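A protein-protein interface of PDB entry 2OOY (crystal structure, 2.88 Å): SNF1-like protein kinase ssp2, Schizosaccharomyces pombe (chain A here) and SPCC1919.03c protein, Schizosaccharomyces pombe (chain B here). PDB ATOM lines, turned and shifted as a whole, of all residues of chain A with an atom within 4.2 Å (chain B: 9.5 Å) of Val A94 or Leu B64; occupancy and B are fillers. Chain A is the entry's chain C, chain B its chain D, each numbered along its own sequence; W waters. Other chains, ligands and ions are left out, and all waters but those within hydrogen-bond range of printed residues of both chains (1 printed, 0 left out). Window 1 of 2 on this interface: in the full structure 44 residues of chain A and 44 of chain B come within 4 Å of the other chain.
Asp A93 touches just one residue of chain B: His B63.
Of chain B, only His B63 and Leu B64 come within 4 Å of Val A94.
Of the printed residues of chain B, Leu A124 touches Leu B64, Leu B76 and Ser B77.
Of the printed residues of chain A, Leu B60 touches Phe A15.
Leu B61 touches none of the printed residues of chain A.
Leu B64 touches just these residues of chain A: Phe A15, Gly A16, Val A94, Leu A124 and Cys A127.
Ala B75 touches none of the printed residues of chain A.
Printed residues of chain A within 4 Å of Ser B77: Leu A124 (3.5 Å).
The nearest residue of chain B that does not touch Val A94 is Asn B62 (4.4 Å).
The nearest printed residue of chain B that does not touch Phe A15 is His B63 (4.03 Å).
Of the 11 printed residues of chain A, 8 touch a printed residue of chain B.
Hydrophobic or aromatic side chains of chain A within 4 Å of the printed part of chain B: Phe A15, Val A94, Phe A123 and Leu A124.
Of the 24 printed residues of chain B, 12 touch a printed residue of chain A.
Among the printed residues, 20 pairs touch across the chains.
Among the printed residues, merely in contact across the chains: Phe A15 with Lys B37 (2.9 Å), Leu A124 with Leu B64 (3.5 Å), Phe A15 with Leu B60 (3.5 Å), Phe A15 with Leu B64 (3.5 Å), Leu A124 with Ser B77 (3.5 Å), Phe A15 with Leu B35 (3.6 Å), Val A94 with His B63 (3.6 Å), Cys A127 with Leu B64 (3.7 Å), Phe A15 with Cys B38 (3.7 Å), Phe A123 with Asn B62 (3.7 Å), Lys A95 with Asn B62 (3.7 Å), Gly A16 with Ala B66 (3.8 Å), Leu A124 with Leu B76 (3.8 Å), Phe A15 with Ala B65 (3.8 Å), Phe A15 with Glu B36 (3.95 Å), Lys A95 with His B63 (3.96 Å) and Gly A16 with Ala B65 (3.99 Å).
Water W1 lies within hydrogen-bond range of O of Leu B64 (2.5 Å), OD1 of Asp A93 (2.7 Å), N of Val A94 (2.9 Å) and N of Gly A16 (3.0 Å).
The backbone carbonyl oxygen (O) of Leu B64 is in hydrogen-bond range of the backbone NH (N) of Gly A16 (2.8 Å).
The side-chain carboxylate (OD1) of Asp A93 sits at hydrogen-bond distance from a ring nitrogen (ND1) of His B63 (2.7 Å).
O of Val A94 sits at hydrogen-bond distance from N of Leu B64 (3.0 Å).
The side-chain carboxylate (OE2) of Glu A79 lies within salt-bridge range of the side-chain amino group (NZ) of Lys A95 (3.4 Å).
O of Phe A123 is in hydrogen-bond range of SG of Cys A127 (3.2 Å).
The backbone carbonyl oxygen of Ala B65 lies within hydrogen-bond range of the backbone NH of Ser B77.
The backbone carbonyl oxygen (O) of Leu B76 is in hydrogen-bond range of the backbone NH (N) of Met B91, at 2.6 Å.
The side-chain hydroxyl (OG) of Ser B77 lies within hydrogen-bond range of the backbone carbonyl oxygen (O) of Thr B89.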
ATOM      1  N   PHE A  15      -8.461  24.016  10.425  1.00  0.00           N
ATOM      2  CA  PHE A  15      -7.352  23.493   9.625  1.00  0.00           C
ATOM      3  C   PHE A  15      -7.756  23.048   8.226  1.00  0.00           C
ATOM      4  O   PHE A  15      -8.915  22.730   7.964  1.00  0.00           O
ATOM      5  CB  PHE A  15      -6.611  22.363  10.335  1.00  0.00           C
ATOM      6  CG  PHE A  15      -5.890  22.806  11.597  1.00  0.00           C
ATOM      7  CD1 PHE A  15      -6.588  22.961  12.814  1.00  0.00           C
ATOM      8  CD2 PHE A  15      -4.512  23.079  11.579  1.00  0.00           C
ATOM      9  CE1 PHE A  15      -5.926  23.361  13.958  1.00  0.00           C
ATOM     10  CE2 PHE A  15      -3.824  23.479  12.740  1.00  0.00           C
ATOM     11  CZ  PHE A  15      -4.526  23.621  13.915  1.00  0.00           C
ATOM     12  N   GLY A  16      -6.760  23.056   7.333  1.00  0.00           N
ATOM     13  CA  GLY A  16      -6.857  22.560   5.975  1.00  0.00           C
ATOM     14  C   GLY A  16      -8.005  23.113   5.199  1.00  0.00           C
ATOM     15  O   GLY A  16      -8.449  24.208   5.462  1.00  0.00           O
ATOM     16  N   ILE A  78       5.165  19.405   0.493  1.00  0.00           N
ATOM     17  CA  ILE A  78       3.879  19.566   1.188  1.00  0.00           C
ATOM     18  C   ILE A  78       3.220  18.224   1.279  1.00  0.00           C
ATOM     19  O   ILE A  78       3.111  17.489   0.295  1.00  0.00           O
ATOM     20  CB  ILE A  78       2.847  20.387   0.379  1.00  0.00           C
ATOM     21  CG1 ILE A  78       3.450  21.626  -0.320  1.00  0.00           C
ATOM     22  CG2 ILE A  78       1.603  20.643   1.208  1.00  0.00           C
ATOM     23  CD1 ILE A  78       3.901  22.699   0.549  1.00  0.00           C
ATOM     24  N   GLU A  79       2.735  17.898   2.444  1.00  0.00           N
ATOM     25  CA  GLU A  79       2.134  16.622   2.593  1.00  0.00           C
ATOM     26  C   GLU A  79       0.657  16.864   2.641  1.00  0.00           C
ATOM     27  O   GLU A  79       0.171  17.539   3.523  1.00  0.00           O
ATOM     28  CB  GLU A  79       2.670  15.955   3.842  1.00  0.00           C
ATOM     29  CG  GLU A  79       1.888  14.814   4.260  1.00  0.00           C
ATOM     30  CD  GLU A  79       2.622  13.935   5.239  1.00  0.00           C
ATOM     31  OE1 GLU A  79       3.881  13.865   5.159  1.00  0.00           O
ATOM     32  OE2 GLU A  79       1.918  13.288   6.076  1.00  0.00           O
ATOM     33  N   LEU A  92      -8.919  18.522   3.964  1.00  0.00           N
ATOM     34  CA  LEU A  92      -7.679  18.336   3.314  1.00  0.00           C
ATOM     35  C   LEU A  92      -6.704  19.034   4.209  1.00  0.00           C
ATOM     36  O   LEU A  92      -6.697  20.232   4.244  1.00  0.00           O
ATOM     37  CB  LEU A  92      -7.666  18.947   1.905  1.00  0.00           C
ATOM     38  CG  LEU A  92      -6.379  18.500   1.159  1.00  0.00           C
ATOM     39  CD1 LEU A  92      -6.303  16.963   0.963  1.00  0.00           C
ATOM     40  CD2 LEU A  92      -6.152  19.212  -0.147  1.00  0.00           C
ATOM     41  N   ASP A  93      -5.918  18.285   4.961  1.00  0.00           N
ATOM     42  CA  ASP A  93      -4.932  18.866   5.809  1.00  0.00           C
ATOM     43  C   ASP A  93      -3.694  18.955   4.987  1.00  0.00           C
ATOM     44  O   ASP A  93      -3.225  17.941   4.441  1.00  0.00           O
ATOM     45  CB  ASP A  93      -4.667  17.995   7.052  1.00  0.00           C
ATOM     46  CG  ASP A  93      -3.346  18.347   7.752  1.00  0.00           C
ATOM     47  OD1 ASP A  93      -3.248  19.425   8.407  1.00  0.00           O
ATOM     48  OD2 ASP A  93      -2.380  17.571   7.615  1.00  0.00           O
ATOM     49  N   VAL A  94      -3.142  20.166   4.948  1.00  0.00           N
ATOM     50  CA  VAL A  94      -1.982  20.477   4.162  1.00  0.00           C
ATOM     51  C   VAL A  94      -0.841  20.713   5.112  1.00  0.00           C
ATOM     52  O   VAL A  94      -1.042  21.444   6.040  1.00  0.00           O
ATOM     53  CB  VAL A  94      -2.213  21.815   3.486  1.00  0.00           C
ATOM     54  CG1 VAL A  94      -0.968  22.204   2.632  1.00  0.00           C
ATOM     55  CG2 VAL A  94      -3.535  21.831   2.680  1.00  0.00           C
ATOM     56  N   LYS A  95       0.343  20.150   4.880  1.00  0.00           N
ATOM     57  CA  LYS A  95       1.478  20.364   5.762  1.00  0.00           C
ATOM     58  C   LYS A  95       2.815  20.684   5.102  1.00  0.00           C
ATOM     59  O   LYS A  95       3.346  19.944   4.281  1.00  0.00           O
ATOM     60  CB  LYS A  95       1.620  19.192   6.716  1.00  0.00           C
ATOM     61  CG  LYS A  95       3.042  18.651   6.936  1.00  0.00           C
ATOM     62  CD  LYS A  95       3.058  17.085   7.121  1.00  0.00           C
ATOM     63  CE  LYS A  95       3.017  16.634   8.604  1.00  0.00           C
ATOM     64  NZ  LYS A  95       2.962  15.107   8.774  1.00  0.00           N
ATOM     65  N   PHE A 123       5.528  28.436   1.841  1.00  0.00           N
ATOM     66  CA  PHE A 123       4.484  27.480   2.069  1.00  0.00           C
ATOM     67  C   PHE A 123       3.081  28.047   1.980  1.00  0.00           C
ATOM     68  O   PHE A 123       2.189  27.428   1.378  1.00  0.00           O
ATOM     69  CB  PHE A 123       4.682  26.780   3.387  1.00  0.00           C
ATOM     70  CG  PHE A 123       3.497  26.000   3.833  1.00  0.00           C
ATOM     71  CD1 PHE A 123       3.143  24.833   3.199  1.00  0.00           C
ATOM     72  CD2 PHE A 123       2.726  26.431   4.903  1.00  0.00           C
ATOM     73  CE1 PHE A 123       2.034  24.075   3.618  1.00  0.00           C
ATOM     74  CE2 PHE A 123       1.619  25.674   5.327  1.00  0.00           C
ATOM     75  CZ  PHE A 123       1.284  24.484   4.661  1.00  0.00           C
ATOM     76  N   LEU A 124       2.839  29.207   2.566  1.00  0.00           N
ATOM     77  CA  LEU A 124       1.497  29.725   2.474  1.00  0.00           C
ATOM     78  C   LEU A 124       1.126  30.074   1.041  1.00  0.00           C
ATOM     79  O   LEU A 124       0.045  29.673   0.579  1.00  0.00           O
ATOM     80  CB  LEU A 124       1.262  30.877   3.424  1.00  0.00           C
ATOM     81  CG  LEU A 124       1.007  30.367   4.862  1.00  0.00           C
ATOM     82  CD1 LEU A 124       1.044  31.535   5.882  1.00  0.00           C
ATOM     83  CD2 LEU A 124      -0.307  29.539   4.996  1.00  0.00           C
ATOM     84  N   CYS A 127       0.262  27.363  -0.614  1.00  0.00           N
ATOM     85  CA  CYS A 127      -1.059  26.988  -0.151  1.00  0.00           C
ATOM     86  C   CYS A 127      -2.047  27.795  -0.951  1.00  0.00           C
ATOM     87  O   CYS A 127      -3.041  27.265  -1.429  1.00  0.00           O
ATOM     88  CB  CYS A 127      -1.218  27.170   1.346  1.00  0.00           C
ATOM     89  SG  CYS A 127      -0.452  25.804   2.140  1.00  0.00           S
ATOM     90  N   LEU B  35      -6.243  18.004  15.696  1.00  0.00           N
ATOM     91  CA  LEU B  35      -6.782  18.998  14.743  1.00  0.00           C
ATOM     92  C   LEU B  35      -8.126  19.435  15.253  1.00  0.00           C
ATOM     93  O   LEU B  35      -8.500  19.099  16.366  1.00  0.00           O
ATOM     94  CB  LEU B  35      -6.913  18.459  13.327  1.00  0.00           C
ATOM     95  CG  LEU B  35      -5.550  18.186  12.704  1.00  0.00           C
ATOM     96  CD1 LEU B  35      -5.750  17.209  11.612  1.00  0.00           C
ATOM     97  CD2 LEU B  35      -4.841  19.455  12.202  1.00  0.00           C
ATOM     98  N   GLU B  36      -8.868  20.194  14.478  1.00  0.00           N
ATOM     99  CA  GLU B  36     -10.199  20.500  14.967  1.00  0.00           C
ATOM    100  C   GLU B  36     -10.231  21.677  15.914  1.00  0.00           C
ATOM    101  O   GLU B  36     -11.306  22.055  16.343  1.00  0.00           O
ATOM    102  CB  GLU B  36     -10.757  19.281  15.713  1.00  0.00           C
ATOM    103  CG  GLU B  36     -12.023  19.495  16.512  1.00  0.00           C
ATOM    104  CD  GLU B  36     -12.419  18.244  17.298  1.00  0.00           C
ATOM    105  OE1 GLU B  36     -11.806  17.984  18.364  1.00  0.00           O
ATOM    106  OE2 GLU B  36     -13.343  17.524  16.852  1.00  0.00           O
ATOM    107  N   LYS B  37      -9.084  22.231  16.286  1.00  0.00           N
ATOM    108  CA  LYS B  37      -9.080  23.362  17.192  1.00  0.00           C
ATOM    109  C   LYS B  37      -7.906  24.218  16.750  1.00  0.00           C
ATOM    110  O   LYS B  37      -6.779  23.737  16.728  1.00  0.00           O
ATOM    111  CB  LYS B  37      -8.987  22.905  18.688  1.00  0.00           C
ATOM    112  CG  LYS B  37      -7.564  22.439  19.223  1.00  0.00           C
ATOM    113  CD  LYS B  37      -7.580  21.410  20.415  1.00  0.00           C
ATOM    114  CE  LYS B  37      -7.573  22.049  21.847  1.00  0.00           C
ATOM    115  NZ  LYS B  37      -6.299  21.875  22.676  1.00  0.00           N
ATOM    116  N   CYS B  38      -8.159  25.461  16.352  1.00  0.00           N
ATOM    117  CA  CYS B  38      -7.052  26.366  16.066  1.00  0.00           C
ATOM    118  C   CYS B  38      -6.638  27.132  17.267  1.00  0.00           C
ATOM    119  O   CYS B  38      -7.473  27.611  18.013  1.00  0.00           O
ATOM    120  CB  CYS B  38      -7.423  27.388  15.024  1.00  0.00           C
ATOM    121  SG  CYS B  38      -7.527  26.642  13.521  1.00  0.00           S
ATOM    122  N   LEU B  40      -5.769  29.855  16.880  1.00  0.00           N
ATOM    123  CA  LEU B  40      -6.176  31.201  16.470  1.00  0.00           C
ATOM    124  C   LEU B  40      -7.587  31.606  16.868  1.00  0.00           C
ATOM    125  O   LEU B  40      -7.935  32.780  16.740  1.00  0.00           O
ATOM    126  CB  LEU B  40      -5.991  31.409  14.964  1.00  0.00           C
ATOM    127  CG  LEU B  40      -4.698  32.018  14.414  1.00  0.00           C
ATOM    128  CD1 LEU B  40      -4.569  31.672  12.963  1.00  0.00           C
ATOM    129  CD2 LEU B  40      -4.651  33.533  14.612  1.00  0.00           C
ATOM    130  N   VAL B  59       2.945  19.190  17.354  1.00  0.00           N
ATOM    131  CA  VAL B  59       2.875  18.248  16.220  1.00  0.00           C
ATOM    132  C   VAL B  59       2.145  18.851  15.051  1.00  0.00           C
ATOM    133  O   VAL B  59       2.505  18.607  13.894  1.00  0.00           O
ATOM    134  CB  VAL B  59       2.311  16.844  16.559  1.00  0.00           C
ATOM    135  CG1 VAL B  59       0.781  16.836  16.487  1.00  0.00           C
ATOM    136  CG2 VAL B  59       2.975  15.762  15.621  1.00  0.00           C
ATOM    137  N   LEU B  60       1.120  19.634  15.367  1.00  0.00           N
ATOM    138  CA  LEU B  60       0.338  20.291  14.349  1.00  0.00           C
ATOM    139  C   LEU B  60       0.946  21.676  14.105  1.00  0.00           C
ATOM    140  O   LEU B  60       0.262  22.715  14.119  1.00  0.00           O
ATOM    141  CB  LEU B  60      -1.149  20.278  14.706  1.00  0.00           C
ATOM    142  CG  LEU B  60      -2.001  21.384  15.304  1.00  0.00           C
ATOM    143  CD1 LEU B  60      -3.355  20.772  15.534  1.00  0.00           C
ATOM    144  CD2 LEU B  60      -1.461  21.939  16.616  1.00  0.00           C
ATOM    145  N   LEU B  61       2.257  21.649  13.860  1.00  0.00           N
ATOM    146  CA  LEU B  61       3.044  22.826  13.750  1.00  0.00           C
ATOM    147  C   LEU B  61       2.772  23.501  12.447  1.00  0.00           C
ATOM    148  O   LEU B  61       1.880  24.341  12.373  1.00  0.00           O
ATOM    149  CB  LEU B  61       4.500  22.470  13.877  1.00  0.00           C
ATOM    150  CG  LEU B  61       5.264  23.605  14.521  1.00  0.00           C
ATOM    151  CD1 LEU B  61       4.305  24.762  14.911  1.00  0.00           C
ATOM    152  CD2 LEU B  61       6.036  23.075  15.717  1.00  0.00           C
ATOM    153  N   ASN B  62       3.491  23.135  11.404  1.00  0.00           N
ATOM    154  CA  ASN B  62       3.415  23.934  10.215  1.00  0.00           C
ATOM    155  C   ASN B  62       2.285  23.489   9.286  1.00  0.00           C
ATOM    156  O   ASN B  62       2.491  22.929   8.229  1.00  0.00           O
ATOM    157  CB  ASN B  62       4.771  23.998   9.531  1.00  0.00           C
ATOM    158  CG  ASN B  62       5.083  25.399   9.013  1.00  0.00           C
ATOM    159  OD1 ASN B  62       6.130  25.960   9.295  1.00  0.00           O
ATOM    160  ND2 ASN B  62       4.151  25.969   8.276  1.00  0.00           N
ATOM    161  N   HIS B  63       1.069  23.756   9.692  1.00  0.00           N
ATOM    162  CA  HIS B  63      -0.063  23.201   8.998  1.00  0.00           C
ATOM    163  C   HIS B  63      -0.993  24.302   8.471  1.00  0.00           C
ATOM    164  O   HIS B  63      -1.104  25.395   9.062  1.00  0.00           O
ATOM    165  CB  HIS B  63      -0.876  22.360   9.987  1.00  0.00           C
ATOM    166  CG  HIS B  63      -0.335  20.998  10.212  1.00  0.00           C
ATOM    167  ND1 HIS B  63      -1.048  19.863   9.887  1.00  0.00           N
ATOM    168  CD2 HIS B  63       0.847  20.576  10.719  1.00  0.00           C
ATOM    169  CE1 HIS B  63      -0.317  18.796  10.166  1.00  0.00           C
ATOM    170  NE2 HIS B  63       0.832  19.200  10.683  1.00  0.00           N
ATOM    171  N   LEU B  64      -1.735  23.992   7.425  1.00  0.00           N
ATOM    172  CA  LEU B  64      -2.520  25.011   6.847  1.00  0.00           C
ATOM    173  C   LEU B  64      -3.786  25.128   7.636  1.00  0.00           C
ATOM    174  O   LEU B  64      -4.277  24.136   8.077  1.00  0.00           O
ATOM    175  CB  LEU B  64      -2.794  24.717   5.384  1.00  0.00           C
ATOM    176  CG  LEU B  64      -3.586  25.876   4.841  1.00  0.00           C
ATOM    177  CD1 LEU B  64      -2.743  27.071   4.976  1.00  0.00           C
ATOM    178  CD2 LEU B  64      -3.874  25.593   3.462  1.00  0.00           C
ATOM    179  N   ALA B  65      -4.277  26.352   7.814  1.00  0.00           N
ATOM    180  CA  ALA B  65      -5.552  26.684   8.460  1.00  0.00           C
ATOM    181  C   ALA B  65      -6.108  27.837   7.680  1.00  0.00           C
ATOM    182  O   ALA B  65      -5.333  28.678   7.249  1.00  0.00           O
ATOM    183  CB  ALA B  65      -5.324  27.142   9.846  1.00  0.00           C
ATOM    184  N   ALA B  66      -7.419  27.906   7.514  1.00  0.00           N
ATOM    185  CA  ALA B  66      -8.009  28.803   6.537  1.00  0.00           C
ATOM    186  C   ALA B  66      -9.168  29.375   7.263  1.00  0.00           C
ATOM    187  O   ALA B  66      -9.545  28.833   8.299  1.00  0.00           O
ATOM    188  CB  ALA B  66      -8.489  28.022   5.258  1.00  0.00           C
ATOM    189  N   ALA B  67      -9.756  30.447   6.738  1.00  0.00           N
ATOM    190  CA  ALA B  67     -10.992  30.987   7.317  1.00  0.00           C
ATOM    191  C   ALA B  67     -11.794  31.783   6.293  1.00  0.00           C
ATOM    192  O   ALA B  67     -11.221  32.345   5.344  1.00  0.00           O
ATOM    193  CB  ALA B  67     -10.683  31.840   8.517  1.00  0.00           C
ATOM    194  N   LEU B  74      -8.545  35.248   0.235  1.00  0.00           N
ATOM    195  CA  LEU B  74      -8.163  34.066   1.005  1.00  0.00           C
ATOM    196  C   LEU B  74      -7.560  34.483   2.317  1.00  0.00           C
ATOM    197  O   LEU B  74      -6.815  35.458   2.383  1.00  0.00           O
ATOM    198  CB  LEU B  74      -7.108  33.225   0.267  1.00  0.00           C
ATOM    199  CG  LEU B  74      -7.447  32.313  -0.953  1.00  0.00           C
ATOM    200  CD1 LEU B  74      -6.210  31.604  -1.578  1.00  0.00           C
ATOM    201  CD2 LEU B  74      -8.480  31.273  -0.574  1.00  0.00           C
ATOM    202  N   ALA B  75      -7.849  33.702   3.359  1.00  0.00           N
ATOM    203  CA  ALA B  75      -7.355  33.898   4.728  1.00  0.00           C
ATOM    204  C   ALA B  75      -6.528  32.686   5.122  1.00  0.00           C
ATOM    205  O   ALA B  75      -7.024  31.664   5.527  1.00  0.00           O
ATOM    206  CB  ALA B  75      -8.537  34.061   5.644  1.00  0.00           C
ATOM    207  N   LEU B  76      -5.239  32.775   4.956  1.00  0.00           N
ATOM    208  CA  LEU B  76      -4.416  31.598   5.216  1.00  0.00           C
ATOM    209  C   LEU B  76      -3.499  31.824   6.369  1.00  0.00           C
ATOM    210  O   LEU B  76      -3.079  32.954   6.653  1.00  0.00           O
ATOM    211  CB  LEU B  76      -3.632  31.146   3.970  1.00  0.00           C
ATOM    212  CG  LEU B  76      -4.525  31.011   2.707  1.00  0.00           C
ATOM    213  CD1 LEU B  76      -3.701  30.695   1.511  1.00  0.00           C
ATOM    214  CD2 LEU B  76      -5.620  29.950   2.834  1.00  0.00           C
ATOM    215  N   SER B  77      -3.193  30.727   7.034  1.00  0.00           N
ATOM    216  CA  SER B  77      -2.481  30.812   8.276  1.00  0.00           C
ATOM    217  C   SER B  77      -1.569  29.654   8.510  1.00  0.00           C
ATOM    218  O   SER B  77      -1.851  28.562   8.011  1.00  0.00           O
ATOM    219  CB  SER B  77      -3.442  30.760   9.424  1.00  0.00           C
ATOM    220  OG  SER B  77      -2.594  30.876  10.532  1.00  0.00           O
ATOM    221  N   ALA B  78      -0.520  29.879   9.300  1.00  0.00           N
ATOM    222  CA  ALA B  78       0.266  28.776   9.788  1.00  0.00           C
ATOM    223  C   ALA B  78       1.216  29.155  10.922  1.00  0.00           C
ATOM    224  O   ALA B  78       1.811  30.249  10.919  1.00  0.00           O
ATOM    225  CB  ALA B  78       1.021  28.093   8.661  1.00  0.00           C
ATOM    226  N   THR B  79       1.347  28.243  11.887  1.00  0.00           N
ATOM    227  CA  THR B  79       2.184  28.499  13.002  1.00  0.00           C
ATOM    228  C   THR B  79       3.546  27.900  12.725  1.00  0.00           C
ATOM    229  O   THR B  79       3.674  26.701  12.467  1.00  0.00           O
ATOM    230  CB  THR B  79       1.589  27.951  14.313  1.00  0.00           C
ATOM    231  OG1 THR B  79       0.385  28.650  14.628  1.00  0.00           O
ATOM    232  CG2 THR B  79       2.540  28.215  15.422  1.00  0.00           C
ATOM    233  N   THR B  88       2.385  32.808  14.573  1.00  0.00           N
ATOM    234  CA  THR B  88       1.309  32.215  13.820  1.00  0.00           C
ATOM    235  C   THR B  88       0.954  33.255  12.839  1.00  0.00           C
ATOM    236  O   THR B  88       0.258  34.199  13.176  1.00  0.00           O
ATOM    237  CB  THR B  88       0.093  31.854  14.654  1.00  0.00           C
ATOM    238  OG1 THR B  88       0.491  30.929  15.665  1.00  0.00           O
ATOM    239  CG2 THR B  88      -0.909  31.176  13.750  1.00  0.00           C
ATOM    240  N   THR B  89       1.496  33.106  11.643  1.00  0.00           N
ATOM    241  CA  THR B  89       1.268  34.073  10.603  1.00  0.00           C
ATOM    242  C   THR B  89      -0.106  33.823  10.014  1.00  0.00           C
ATOM    243  O   THR B  89      -0.587  32.670   9.953  1.00  0.00           O
ATOM    244  CB  THR B  89       2.283  33.927   9.532  1.00  0.00           C
ATOM    245  OG1 THR B  89       3.513  33.462  10.108  1.00  0.00           O
ATOM    246  CG2 THR B  89       2.499  35.253   8.846  1.00  0.00           C
ATOM    247  N   ALA B  90      -0.766  34.902   9.631  1.00  0.00           N
ATOM    248  CA  ALA B  90      -2.100  34.791   9.090  1.00  0.00           C
ATOM    249  C   ALA B  90      -2.263  35.834   7.996  1.00  0.00           C
ATOM    250  O   ALA B  90      -2.467  37.025   8.295  1.00  0.00           O
ATOM    251  CB  ALA B  90      -3.154  34.956  10.176  1.00  0.00           C
ATOM    252  N   MET B  91      -2.144  35.383   6.740  1.00  0.00           N
ATOM    253  CA  MET B  91      -2.066  36.289   5.609  1.00  0.00           C
ATOM    254  C   MET B  91      -3.418  36.392   5.045  1.00  0.00           C
ATOM    255  O   MET B  91      -4.132  35.387   4.961  1.00  0.00           O
ATOM    256  CB  MET B  91      -1.196  35.752   4.489  1.00  0.00           C
ATOM    257  CG  MET B  91      -1.059  36.652   3.305  1.00  0.00           C
ATOM    258  SD  MET B  91       0.225  35.895   2.348  1.00  0.00           S
ATOM    259  CE  MET B  91      -0.589  34.357   1.959  1.00  0.00           C
HETATM  260  O   HOH W   1      -4.022  21.757   7.198  1.00  0.00           O
